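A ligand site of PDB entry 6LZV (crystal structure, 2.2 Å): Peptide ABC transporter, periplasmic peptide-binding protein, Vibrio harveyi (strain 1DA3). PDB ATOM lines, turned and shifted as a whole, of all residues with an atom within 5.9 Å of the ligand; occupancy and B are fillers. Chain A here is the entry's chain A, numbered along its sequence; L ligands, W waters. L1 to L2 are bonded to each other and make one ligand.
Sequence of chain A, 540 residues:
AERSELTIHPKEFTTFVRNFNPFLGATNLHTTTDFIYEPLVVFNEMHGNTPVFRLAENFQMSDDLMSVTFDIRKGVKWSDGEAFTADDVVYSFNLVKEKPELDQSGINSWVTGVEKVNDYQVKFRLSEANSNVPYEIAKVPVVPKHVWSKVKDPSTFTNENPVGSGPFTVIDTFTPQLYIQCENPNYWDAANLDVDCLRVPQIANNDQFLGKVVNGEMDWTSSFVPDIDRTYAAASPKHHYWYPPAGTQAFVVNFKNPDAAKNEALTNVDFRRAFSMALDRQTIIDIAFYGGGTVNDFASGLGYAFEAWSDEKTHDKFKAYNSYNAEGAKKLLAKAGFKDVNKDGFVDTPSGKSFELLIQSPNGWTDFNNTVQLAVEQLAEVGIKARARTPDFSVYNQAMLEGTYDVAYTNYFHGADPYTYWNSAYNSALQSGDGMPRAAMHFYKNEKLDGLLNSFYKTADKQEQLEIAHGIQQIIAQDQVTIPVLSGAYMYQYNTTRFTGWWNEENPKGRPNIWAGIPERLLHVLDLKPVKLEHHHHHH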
ATOM      1  N   HIS A   9     -18.806  -6.141  12.995  1.00  0.00           N
ATOM      2  CA  HIS A   9     -18.824  -5.499  11.684  1.00  0.00           C
ATOM      3  C   HIS A   9     -17.853  -6.147  10.699  1.00  0.00           C
ATOM      4  O   HIS A   9     -16.747  -5.625  10.476  1.00  0.00           O
ATOM      5  CB  HIS A   9     -18.481  -4.013  11.801  1.00  0.00           C
ATOM      6  CG  HIS A   9     -18.499  -3.299  10.500  1.00  0.00           C
ATOM      7  ND1 HIS A   9     -19.430  -3.575   9.519  1.00  0.00           N
ATOM      8  CD2 HIS A   9     -17.697  -2.336   9.989  1.00  0.00           C
ATOM      9  CE1 HIS A   9     -19.214  -2.806   8.466  1.00  0.00           C
ATOM     10  NE2 HIS A   9     -18.173  -2.036   8.734  1.00  0.00           N
ATOM     11  N   PRO A  10     -18.257  -7.277  10.082  1.00  0.00           N
ATOM     12  CA  PRO A  10     -17.332  -7.996   9.202  1.00  0.00           C
ATOM     13  C   PRO A  10     -17.179  -7.419   7.790  1.00  0.00           C
ATOM     14  O   PRO A  10     -16.168  -7.683   7.139  1.00  0.00           O
ATOM     15  CB  PRO A  10     -17.938  -9.409   9.151  1.00  0.00           C
ATOM     16  CG  PRO A  10     -19.383  -9.215   9.436  1.00  0.00           C
ATOM     17  CD  PRO A  10     -19.492  -8.048  10.353  1.00  0.00           C
ATOM     18  N   LYS A  11     -18.138  -6.632   7.336  1.00  0.00           N
ATOM     19  CA  LYS A  11     -18.187  -6.260   5.932  1.00  0.00           C
ATOM     20  C   LYS A  11     -19.135  -5.103   5.718  1.00  0.00           C
ATOM     21  O   LYS A  11     -20.225  -5.089   6.280  1.00  0.00           O
ATOM     22  CB  LYS A  11     -18.631  -7.470   5.067  1.00  0.00           C
ATOM     23  CG  LYS A  11     -18.594  -7.223   3.539  1.00  0.00           C
ATOM     24  CD  LYS A  11     -17.177  -7.283   3.002  1.00  0.00           C
ATOM     25  CE  LYS A  11     -17.054  -6.618   1.630  1.00  0.00           C
ATOM     26  NZ  LYS A  11     -17.821  -7.332   0.603  1.00  0.00           N
ATOM     27  N   GLU A  12     -18.718  -4.121   4.922  1.00  0.00           N
ATOM     28  CA  GLU A  12     -19.596  -2.996   4.612  1.00  0.00           C
ATOM     29  C   GLU A  12     -20.687  -3.389   3.595  1.00  0.00           C
ATOM     30  O   GLU A  12     -20.466  -4.168   2.684  1.00  0.00           O
ATOM     31  CB  GLU A  12     -18.782  -1.766   4.144  1.00  0.00           C
ATOM     32  CG  GLU A  12     -17.623  -2.023   3.196  1.00  0.00           C
ATOM     33  CD  GLU A  12     -16.342  -2.496   3.893  1.00  0.00           C
ATOM     34  OE1 GLU A  12     -16.117  -3.712   3.848  1.00  0.00           O
ATOM     35  OE2 GLU A  12     -15.561  -1.680   4.462  1.00  0.00           O
ATOM     36  N   HIS A  30     -21.670 -11.897   5.620  1.00  0.00           N
ATOM     37  CA  HIS A  30     -20.351 -12.325   6.028  1.00  0.00           C
ATOM     38  C   HIS A  30     -20.271 -12.856   7.455  1.00  0.00           C
ATOM     39  O   HIS A  30     -19.202 -12.837   8.065  1.00  0.00           O
ATOM     40  CB  HIS A  30     -19.380 -11.172   5.827  1.00  0.00           C
ATOM     41  CG  HIS A  30     -18.970 -11.017   4.398  1.00  0.00           C
ATOM     42  ND1 HIS A  30     -17.671 -10.762   4.013  1.00  0.00           N
ATOM     43  CD2 HIS A  30     -19.690 -11.106   3.255  1.00  0.00           C
ATOM     44  CE1 HIS A  30     -17.609 -10.690   2.695  1.00  0.00           C
ATOM     45  NE2 HIS A  30     -18.821 -10.887   2.207  1.00  0.00           N
ATOM     46  N   ASN A 206     -15.927   3.746   5.636  1.00  0.00           N
ATOM     47  CA  ASN A 206     -15.155   4.033   6.848  1.00  0.00           C
ATOM     48  C   ASN A 206     -15.664   5.290   7.554  1.00  0.00           C
ATOM     49  O   ASN A 206     -15.476   5.444   8.756  1.00  0.00           O
ATOM     50  CB  ASN A 206     -13.672   4.185   6.538  1.00  0.00           C
ATOM     51  CG  ASN A 206     -13.023   2.871   6.117  1.00  0.00           C
ATOM     52  OD1 ASN A 206     -13.612   1.782   6.270  1.00  0.00           O
ATOM     53  ND2 ASN A 206     -11.820   2.959   5.585  1.00  0.00           N
ATOM     54  N   THR A 221     -14.606  -5.043  15.978  1.00  0.00           N
ATOM     55  CA  THR A 221     -14.478  -4.565  14.605  1.00  0.00           C
ATOM     56  C   THR A 221     -13.037  -4.667  14.073  1.00  0.00           C
ATOM     57  O   THR A 221     -12.098  -4.876  14.831  1.00  0.00           O
ATOM     58  CB  THR A 221     -14.979  -3.133  14.496  1.00  0.00           C
ATOM     59  OG1 THR A 221     -14.165  -2.280  15.301  1.00  0.00           O
ATOM     60  CG2 THR A 221     -16.440  -3.015  14.942  1.00  0.00           C
ATOM     61  N   SER A 222     -12.904  -4.521  12.753  1.00  0.00           N
ATOM     62  CA  SER A 222     -11.628  -4.680  12.065  1.00  0.00           C
ATOM     63  C   SER A 222     -11.470  -3.694  10.915  1.00  0.00           C
ATOM     64  O   SER A 222     -10.840  -4.019   9.923  1.00  0.00           O
ATOM     65  CB  SER A 222     -11.500  -6.104  11.525  1.00  0.00           C
ATOM     66  OG  SER A 222     -11.370  -7.037  12.556  1.00  0.00           O
ATOM     67  N   SER A 223     -12.056  -2.503  11.068  1.00  0.00           N
ATOM     68  CA  SER A 223     -12.021  -1.455  10.052  1.00  0.00           C
ATOM     69  C   SER A 223     -10.814  -0.555  10.170  1.00  0.00           C
ATOM     70  O   SER A 223     -10.160  -0.523  11.193  1.00  0.00           O
ATOM     71  CB  SER A 223     -13.287  -0.590  10.127  1.00  0.00           C
ATOM     72  OG  SER A 223     -14.424  -1.321   9.728  1.00  0.00           O
ATOM     73  N   PHE A 224     -10.541   0.213   9.107  1.00  0.00           N
ATOM     74  CA  PHE A 224      -9.559   1.270   9.214  1.00  0.00           C
ATOM     75  C   PHE A 224     -10.115   2.432  10.028  1.00  0.00           C
ATOM     76  O   PHE A 224     -11.250   2.858   9.830  1.00  0.00           O
ATOM     77  CB  PHE A 224      -9.134   1.787   7.842  1.00  0.00           C
ATOM     78  CG  PHE A 224      -8.201   2.983   7.913  1.00  0.00           C
ATOM     79  CD1 PHE A 224      -6.926   2.840   8.420  1.00  0.00           C
ATOM     80  CD2 PHE A 224      -8.610   4.232   7.483  1.00  0.00           C
ATOM     81  CE1 PHE A 224      -6.077   3.921   8.493  1.00  0.00           C
ATOM     82  CE2 PHE A 224      -7.761   5.313   7.556  1.00  0.00           C
ATOM     83  CZ  PHE A 224      -6.483   5.156   8.059  1.00  0.00           C
ATOM     84  N   GLN A 249       0.671  -5.360   0.716  1.00  0.00           N
ATOM     85  CA  GLN A 249      -0.192  -4.550  -0.138  1.00  0.00           C
ATOM     86  C   GLN A 249       0.641  -4.057  -1.292  1.00  0.00           C
ATOM     87  O   GLN A 249       1.842  -3.765  -1.112  1.00  0.00           O
ATOM     88  CB  GLN A 249      -0.796  -3.387   0.644  1.00  0.00           C
ATOM     89  CG  GLN A 249      -1.594  -3.888   1.842  1.00  0.00           C
ATOM     90  CD  GLN A 249      -2.148  -2.756   2.680  1.00  0.00           C
ATOM     91  OE1 GLN A 249      -2.295  -1.631   2.201  1.00  0.00           O
ATOM     92  NE2 GLN A 249      -2.423  -3.052   3.940  1.00  0.00           N
ATOM     93  N   PHE A 289      -1.732   5.614   6.583  1.00  0.00           N
ATOM     94  CA  PHE A 289      -2.001   4.560   7.575  1.00  0.00           C
ATOM     95  C   PHE A 289      -1.618   4.998   8.991  1.00  0.00           C
ATOM     96  O   PHE A 289      -1.698   4.213   9.932  1.00  0.00           O
ATOM     97  CB  PHE A 289      -1.252   3.277   7.209  1.00  0.00           C
ATOM     98  CG  PHE A 289      -1.704   2.658   5.922  1.00  0.00           C
ATOM     99  CD1 PHE A 289      -1.173   3.075   4.715  1.00  0.00           C
ATOM    100  CD2 PHE A 289      -2.684   1.680   5.922  1.00  0.00           C
ATOM    101  CE1 PHE A 289      -1.606   2.512   3.525  1.00  0.00           C
ATOM    102  CE2 PHE A 289      -3.115   1.114   4.741  1.00  0.00           C
ATOM    103  CZ  PHE A 289      -2.577   1.537   3.545  1.00  0.00           C
ATOM    104  N   GLY A 364     -14.945   3.522  -0.213  1.00  0.00           N
ATOM    105  CA  GLY A 364     -15.116   3.372   1.218  1.00  0.00           C
ATOM    106  C   GLY A 364     -13.870   2.917   1.958  1.00  0.00           C
ATOM    107  O   GLY A 364     -13.765   3.125   3.178  1.00  0.00           O
ATOM    108  N   TRP A 365     -12.928   2.280   1.256  1.00  0.00           N
ATOM    109  CA  TRP A 365     -11.712   1.830   1.939  1.00  0.00           C
ATOM    110  C   TRP A 365     -10.727   3.005   1.984  1.00  0.00           C
ATOM    111  O   TRP A 365      -9.776   3.061   1.213  1.00  0.00           O
ATOM    112  CB  TRP A 365     -11.052   0.624   1.252  1.00  0.00           C
ATOM    113  CG  TRP A 365     -11.890  -0.663   1.193  1.00  0.00           C
ATOM    114  CD1 TRP A 365     -13.242  -0.776   1.385  1.00  0.00           C
ATOM    115  CD2 TRP A 365     -11.414  -1.989   0.904  1.00  0.00           C
ATOM    116  NE1 TRP A 365     -13.637  -2.084   1.221  1.00  0.00           N
ATOM    117  CE2 TRP A 365     -12.539  -2.858   0.927  1.00  0.00           C
ATOM    118  CE3 TRP A 365     -10.156  -2.530   0.606  1.00  0.00           C
ATOM    119  CZ2 TRP A 365     -12.441  -4.234   0.669  1.00  0.00           C
ATOM    120  CZ3 TRP A 365     -10.059  -3.895   0.362  1.00  0.00           C
ATOM    121  CH2 TRP A 365     -11.197  -4.732   0.397  1.00  0.00           C
ATOM    122  N   THR A 366     -10.981   3.957   2.876  1.00  0.00           N
ATOM    123  CA  THR A 366     -10.330   5.254   2.771  1.00  0.00           C
ATOM    124  C   THR A 366      -8.793   5.239   2.879  1.00  0.00           C
ATOM    125  O   THR A 366      -8.139   6.054   2.248  1.00  0.00           O
ATOM    126  CB  THR A 366     -10.873   6.209   3.820  1.00  0.00           C
ATOM    127  OG1 THR A 366     -10.932   5.519   5.069  1.00  0.00           O
ATOM    128  CG2 THR A 366     -12.289   6.653   3.423  1.00  0.00           C
ATOM    129  N   ASP A 367      -8.236   4.342   3.688  1.00  0.00           N
ATOM    130  CA  ASP A 367      -6.785   4.208   3.767  1.00  0.00           C
ATOM    131  C   ASP A 367      -6.169   3.882   2.387  1.00  0.00           C
ATOM    132  O   ASP A 367      -5.112   4.422   2.030  1.00  0.00           O
ATOM    133  CB  ASP A 367      -6.362   3.143   4.815  1.00  0.00           C
ATOM    134  CG  ASP A 367      -7.152   1.826   4.738  1.00  0.00           C
ATOM    135  OD1 ASP A 367      -8.313   1.798   4.268  1.00  0.00           O
ATOM    136  OD2 ASP A 367      -6.618   0.791   5.206  1.00  0.00           O
ATOM    137  N   PHE A 368      -6.857   3.035   1.615  1.00  0.00           N
ATOM    138  CA  PHE A 368      -6.394   2.636   0.283  1.00  0.00           C
ATOM    139  C   PHE A 368      -6.639   3.741  -0.721  1.00  0.00           C
ATOM    140  O   PHE A 368      -5.834   3.920  -1.632  1.00  0.00           O
ATOM    141  CB  PHE A 368      -7.094   1.359  -0.208  1.00  0.00           C
ATOM    142  CG  PHE A 368      -6.623   0.079   0.455  1.00  0.00           C
ATOM    143  CD1 PHE A 368      -5.907   0.103   1.633  1.00  0.00           C
ATOM    144  CD2 PHE A 368      -6.935  -1.148  -0.111  1.00  0.00           C
ATOM    145  CE1 PHE A 368      -5.491  -1.082   2.248  1.00  0.00           C
ATOM    146  CE2 PHE A 368      -6.538  -2.328   0.476  1.00  0.00           C
ATOM    147  CZ  PHE A 368      -5.806  -2.303   1.663  1.00  0.00           C
ATOM    148  N   THR A 410      -4.227  -3.229  -3.994  1.00  0.00           N
ATOM    149  CA  THR A 410      -4.899  -4.252  -3.218  1.00  0.00           C
ATOM    150  C   THR A 410      -4.070  -4.836  -2.094  1.00  0.00           C
ATOM    151  O   THR A 410      -2.846  -4.775  -2.100  1.00  0.00           O
ATOM    152  CB  THR A 410      -5.349  -5.432  -4.084  1.00  0.00           C
ATOM    153  OG1 THR A 410      -5.832  -6.477  -3.220  1.00  0.00           O
ATOM    154  CG2 THR A 410      -4.172  -5.986  -4.866  1.00  0.00           C
ATOM    155  N   ASN A 411      -4.766  -5.419  -1.126  1.00  0.00           N
ATOM    156  CA  ASN A 411      -4.130  -6.243  -0.121  1.00  0.00           C
ATOM    157  C   ASN A 411      -4.303  -7.716  -0.443  1.00  0.00           C
ATOM    158  O   ASN A 411      -5.149  -8.090  -1.255  1.00  0.00           O
ATOM    159  CB  ASN A 411      -4.677  -5.956   1.278  1.00  0.00           C
ATOM    160  CG  ASN A 411      -6.185  -6.115   1.358  1.00  0.00           C
ATOM    161  OD1 ASN A 411      -6.872  -6.150   0.351  1.00  0.00           O
ATOM    162  ND2 ASN A 411      -6.705  -6.200   2.594  1.00  0.00           N
ATOM    163  N   TYR A 412      -3.494  -8.553   0.202  1.00  0.00           N
ATOM    164  CA  TYR A 412      -3.567  -9.997   0.038  1.00  0.00           C
ATOM    165  C   TYR A 412      -3.799 -10.688   1.358  1.00  0.00           C
ATOM    166  O   TYR A 412      -3.447 -10.158   2.416  1.00  0.00           O
ATOM    167  CB  TYR A 412      -2.282 -10.547  -0.551  1.00  0.00           C
ATOM    168  CG  TYR A 412      -1.939  -9.968  -1.880  1.00  0.00           C
ATOM    169  CD1 TYR A 412      -1.227  -8.777  -1.973  1.00  0.00           C
ATOM    170  CD2 TYR A 412      -2.299 -10.620  -3.055  1.00  0.00           C
ATOM    171  CE1 TYR A 412      -0.876  -8.254  -3.214  1.00  0.00           C
ATOM    172  CE2 TYR A 412      -1.968 -10.098  -4.283  1.00  0.00           C
ATOM    173  CZ  TYR A 412      -1.249  -8.929  -4.351  1.00  0.00           C
ATOM    174  OH  TYR A 412      -0.921  -8.428  -5.584  1.00  0.00           O
ATOM    175  N   PHE A 413      -4.321 -11.898   1.287  1.00  0.00           N
ATOM    176  CA  PHE A 413      -4.360 -12.704   2.488  1.00  0.00           C
ATOM    177  C   PHE A 413      -2.947 -13.116   2.853  1.00  0.00           C
ATOM    178  O   PHE A 413      -2.049 -13.160   2.010  1.00  0.00           O
ATOM    179  CB  PHE A 413      -5.293 -13.902   2.280  1.00  0.00           C
ATOM    180  CG  PHE A 413      -6.735 -13.520   2.376  1.00  0.00           C
ATOM    181  CD1 PHE A 413      -7.289 -13.162   3.595  1.00  0.00           C
ATOM    182  CD2 PHE A 413      -7.526 -13.450   1.237  1.00  0.00           C
ATOM    183  CE1 PHE A 413      -8.615 -12.774   3.692  1.00  0.00           C
ATOM    184  CE2 PHE A 413      -8.858 -13.070   1.333  1.00  0.00           C
ATOM    185  CZ  PHE A 413      -9.392 -12.728   2.566  1.00  0.00           C
ATOM    186  N   ARG A 438      -9.655 -11.733  -6.547  1.00  0.00           N
ATOM    187  CA  ARG A 438      -8.987 -10.777  -7.426  1.00  0.00           C
ATOM    188  C   ARG A 438      -7.448 -10.879  -7.470  1.00  0.00           C
ATOM    189  O   ARG A 438      -6.814 -10.349  -8.378  1.00  0.00           O
ATOM    190  CB  ARG A 438      -9.365  -9.368  -7.005  1.00  0.00           C
ATOM    191  CG  ARG A 438      -8.720  -8.948  -5.691  1.00  0.00           C
ATOM    192  CD  ARG A 438      -9.405  -7.702  -5.147  1.00  0.00           C
ATOM    193  NE  ARG A 438      -8.871  -7.287  -3.858  1.00  0.00           N
ATOM    194  CZ  ARG A 438      -9.314  -7.723  -2.682  1.00  0.00           C
ATOM    195  NH1 ARG A 438     -10.283  -8.639  -2.657  1.00  0.00           N
ATOM    196  NH2 ARG A 438      -8.773  -7.288  -1.547  1.00  0.00           N
ATOM    197  N   MET A 491      -6.027  -4.698  11.329  1.00  0.00           N
ATOM    198  CA  MET A 491      -6.770  -3.722  12.123  1.00  0.00           C
ATOM    199  C   MET A 491      -7.834  -4.430  12.940  1.00  0.00           C
ATOM    200  O   MET A 491      -8.559  -5.306  12.429  1.00  0.00           O
ATOM    201  CB  MET A 491      -7.417  -2.642  11.255  1.00  0.00           C
ATOM    202  CG  MET A 491      -6.482  -2.046  10.239  1.00  0.00           C
ATOM    203  SD  MET A 491      -6.519  -3.042   8.742  1.00  0.00           S
ATOM    204  CE  MET A 491      -8.090  -2.514   8.037  1.00  0.00           C
ATOM    205  N   TRP A 515     -13.344 -10.379  10.111  1.00  0.00           N
ATOM    206  CA  TRP A 515     -13.621 -10.605   8.684  1.00  0.00           C
ATOM    207  C   TRP A 515     -13.967 -12.056   8.355  1.00  0.00           C
ATOM    208  O   TRP A 515     -13.481 -12.967   9.025  1.00  0.00           O
ATOM    209  CB  TRP A 515     -12.413 -10.212   7.826  1.00  0.00           C
ATOM    210  CG  TRP A 515     -11.938  -8.784   7.968  1.00  0.00           C
ATOM    211  CD1 TRP A 515     -12.700  -7.680   8.201  1.00  0.00           C
ATOM    212  CD2 TRP A 515     -10.585  -8.348   7.898  1.00  0.00           C
ATOM    213  NE1 TRP A 515     -11.894  -6.568   8.270  1.00  0.00           N
ATOM    214  CE2 TRP A 515     -10.584  -6.956   8.091  1.00  0.00           C
ATOM    215  CE3 TRP A 515      -9.369  -8.994   7.673  1.00  0.00           C
ATOM    216  CZ2 TRP A 515      -9.425  -6.209   8.068  1.00  0.00           C
ATOM    217  CZ3 TRP A 515      -8.209  -8.239   7.673  1.00  0.00           C
ATOM    218  CH2 TRP A 515      -8.247  -6.870   7.867  1.00  0.00           C
ATOM    219  N   ALA A 516     -14.781 -12.284   7.337  1.00  0.00           N
ATOM    220  CA  ALA A 516     -14.894 -13.639   6.794  1.00  0.00           C
ATOM    221  C   ALA A 516     -13.554 -13.936   6.151  1.00  0.00           C
ATOM    222  O   ALA A 516     -12.891 -13.027   5.660  1.00  0.00           O
ATOM    223  CB  ALA A 516     -16.029 -13.758   5.789  1.00  0.00           C
HETATM  224  C1  LIG L   1     -11.513  -8.531   3.604  1.00  0.00           C
HETATM  225  C2  LIG L   1     -10.350  -7.656   3.153  1.00  0.00           C
HETATM  226  C3  LIG L   1     -10.305  -6.523   4.150  1.00  0.00           C
HETATM  227  C4  LIG L   1     -11.636  -5.769   4.205  1.00  0.00           C
HETATM  228  C5  LIG L   1     -12.788  -6.766   4.450  1.00  0.00           C
HETATM  229  C6  LIG L   1     -14.170  -6.131   4.543  1.00  0.00           C
HETATM  230  C7  LIG L   1      -8.538  -8.861   2.087  1.00  0.00           C
HETATM  231  C8  LIG L   1      -7.270  -9.645   2.256  1.00  0.00           C
HETATM  232  N1  LIG L   1      -9.082  -8.369   3.195  1.00  0.00           N
HETATM  233  O1  LIG L   1     -11.541  -9.709   2.812  1.00  0.00           O
HETATM  234  O2  LIG L   1      -9.215  -5.707   3.770  1.00  0.00           O
HETATM  235  O3  LIG L   1     -11.622  -4.876   5.297  1.00  0.00           O
HETATM  236  O4  LIG L   1     -12.736  -7.781   3.449  1.00  0.00           O
HETATM  237  O5  LIG L   1     -14.393  -5.345   3.371  1.00  0.00           O
HETATM  238  O6  LIG L   1      -9.027  -8.688   0.988  1.00  0.00           O
HETATM  239  C1  LG2 L   2     -11.604  -3.534   4.894  1.00  0.00           C
HETATM  240  C2  LG2 L   2     -12.135  -2.689   6.036  1.00  0.00           C
HETATM  241  C3  LG2 L   2     -11.934  -1.226   5.687  1.00  0.00           C
HETATM  242  C4  LG2 L   2     -10.479  -0.946   5.313  1.00  0.00           C
HETATM  243  C5  LG2 L   2     -10.121  -1.894   4.182  1.00  0.00           C
HETATM  244  C6  LG2 L   2      -8.695  -1.673   3.691  1.00  0.00           C
HETATM  245  C7  LG2 L   2     -14.000  -3.628   7.380  1.00  0.00           C
HETATM  246  C8  LG2 L   2     -15.500  -3.835   7.425  1.00  0.00           C
HETATM  247  N1  LG2 L   2     -13.544  -2.925   6.320  1.00  0.00           N
HETATM  248  O1  LG2 L   2     -12.282  -0.472   6.846  1.00  0.00           O
HETATM  249  O2  LG2 L   2     -10.306   0.413   4.898  1.00  0.00           O
HETATM  250  O3  LG2 L   2     -10.243  -3.204   4.687  1.00  0.00           O
HETATM  251  O4  LG2 L   2      -7.851  -1.485   4.830  1.00  0.00           O
HETATM  252  O5  LG2 L   2     -13.282  -4.059   8.261  1.00  0.00           O
HETATM  253  O   HOH W   1     -16.088  -3.692   1.025  1.00  0.00           O
HETATM  254  O   HOH W   2     -13.597 -10.960   4.176  1.00  0.00           O
HETATM  255  O   HOH W   3     -14.752  -4.047  10.764  1.00  0.00           O
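O5 of LG2 L2 lies close to N of Ser 223, 3.4 Å away. An oxygen (O1) of LG2 L2 lies within hydrogen-bond range of the backbone NH of Phe 224 (2.9 Å). OD1 of Asp 367 is in hydrogen-bond range of O2 of LG2 L2 (2.5 Å). An oxygen (O5) of LIG L1 lies within hydrogen-bond range of the side-chain carboxylate of Glu 12 (2.4 Å). An oxygen (O5) of LG2 L2 is in hydrogen-bond range of the side-chain hydroxyl of Ser 223, 3.3 Å away. The side-chain amide oxygen (OD1) of Asn 206 is in hydrogen-bond range of an oxygen (O1) of LG2 L2 (2.7 Å). The guanidinium group (NH2) of Arg 438 sits at hydrogen-bond distance from an oxygen (O6) of LIG L1 (2.9 Å). ND2 of Asn 411 sits at hydrogen-bond distance from O2 of LIG L1. An oxygen (O5) of LG2 L2 is in hydrogen-bond range of the indole nitrogen (NE1) of Trp 515 (2.9 Å).
The backbone carbonyl oxygen (O) of Met 491 sits close to the side-chain hydroxyl (OG) of Ser 222. ND2 of Asn 206 lies close to O of Gly 364 (3.1 Å). The side-chain amide nitrogen of Asn 206 sits at hydrogen-bond distance from the side-chain hydroxyl of Thr 366, at 2.8 Å. The side-chain hydroxyl of Thr 410 is in hydrogen-bond range of the guanidinium group of Arg 438, at 3.2 Å. The indole nitrogen (NE1) of Trp 515 sits close to the backbone carbonyl oxygen (O) of Ser 222 (3.2 Å). The side-chain amide oxygen of Asn 411 sits at hydrogen-bond distance from the guanidinium group of Arg 438, 2.9 Å away.
O of Ser 222 lies close to O5 of LG2 L2 (3.0 Å). NE2 of His 9 touches C8 of LG2 L2, 3.5 Å away. O of Pro 10 touches C6 of LIG L1, 3.6 Å away. CD of Lys 11 touches O5 of LIG L1, 3.4 Å away. Trp 365 touches the ligand. Phe 368 touches the ligand. Tyr 412 touches the ligand. CE1 of Phe 413 touches C8 of LIG L1 (3.7 Å). CE of Met 491 touches O4 of LG2 L2, at 3.4 Å. 17 residues have an atom within 4 Å of the ligand: His 9, Pro 10, Lys 11, Glu 12, Asn 206, Ser 222, Ser 223, Phe 224, Trp 365, Asp 367, Phe 368, Asn 411, Tyr 412, Phe 413, Arg 438, Met 491 and Trp 515. The nearest printed residue that does not touch the ligand is Thr 366 (4.1 Å).
Water W2 bridges O of Ala 516 (2.6 Å) and O1 of LIG L1 (2.8 Å). Water W3 lies within hydrogen-bond range of the backbone carbonyl oxygen (O) of His 9, the backbone NH (N) of Ser 222, an oxygen (O5) of LG2 L2 and the side-chain hydroxyl (OG) of Ser 223. Water W1 lies within hydrogen-bond range of the side-chain carboxylate (OE1) of Glu 12 (2.8 Å), the indole nitrogen (NE1) of Trp 365 (2.9 Å) and an oxygen (O5) of LIG L1 (3.3 Å).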
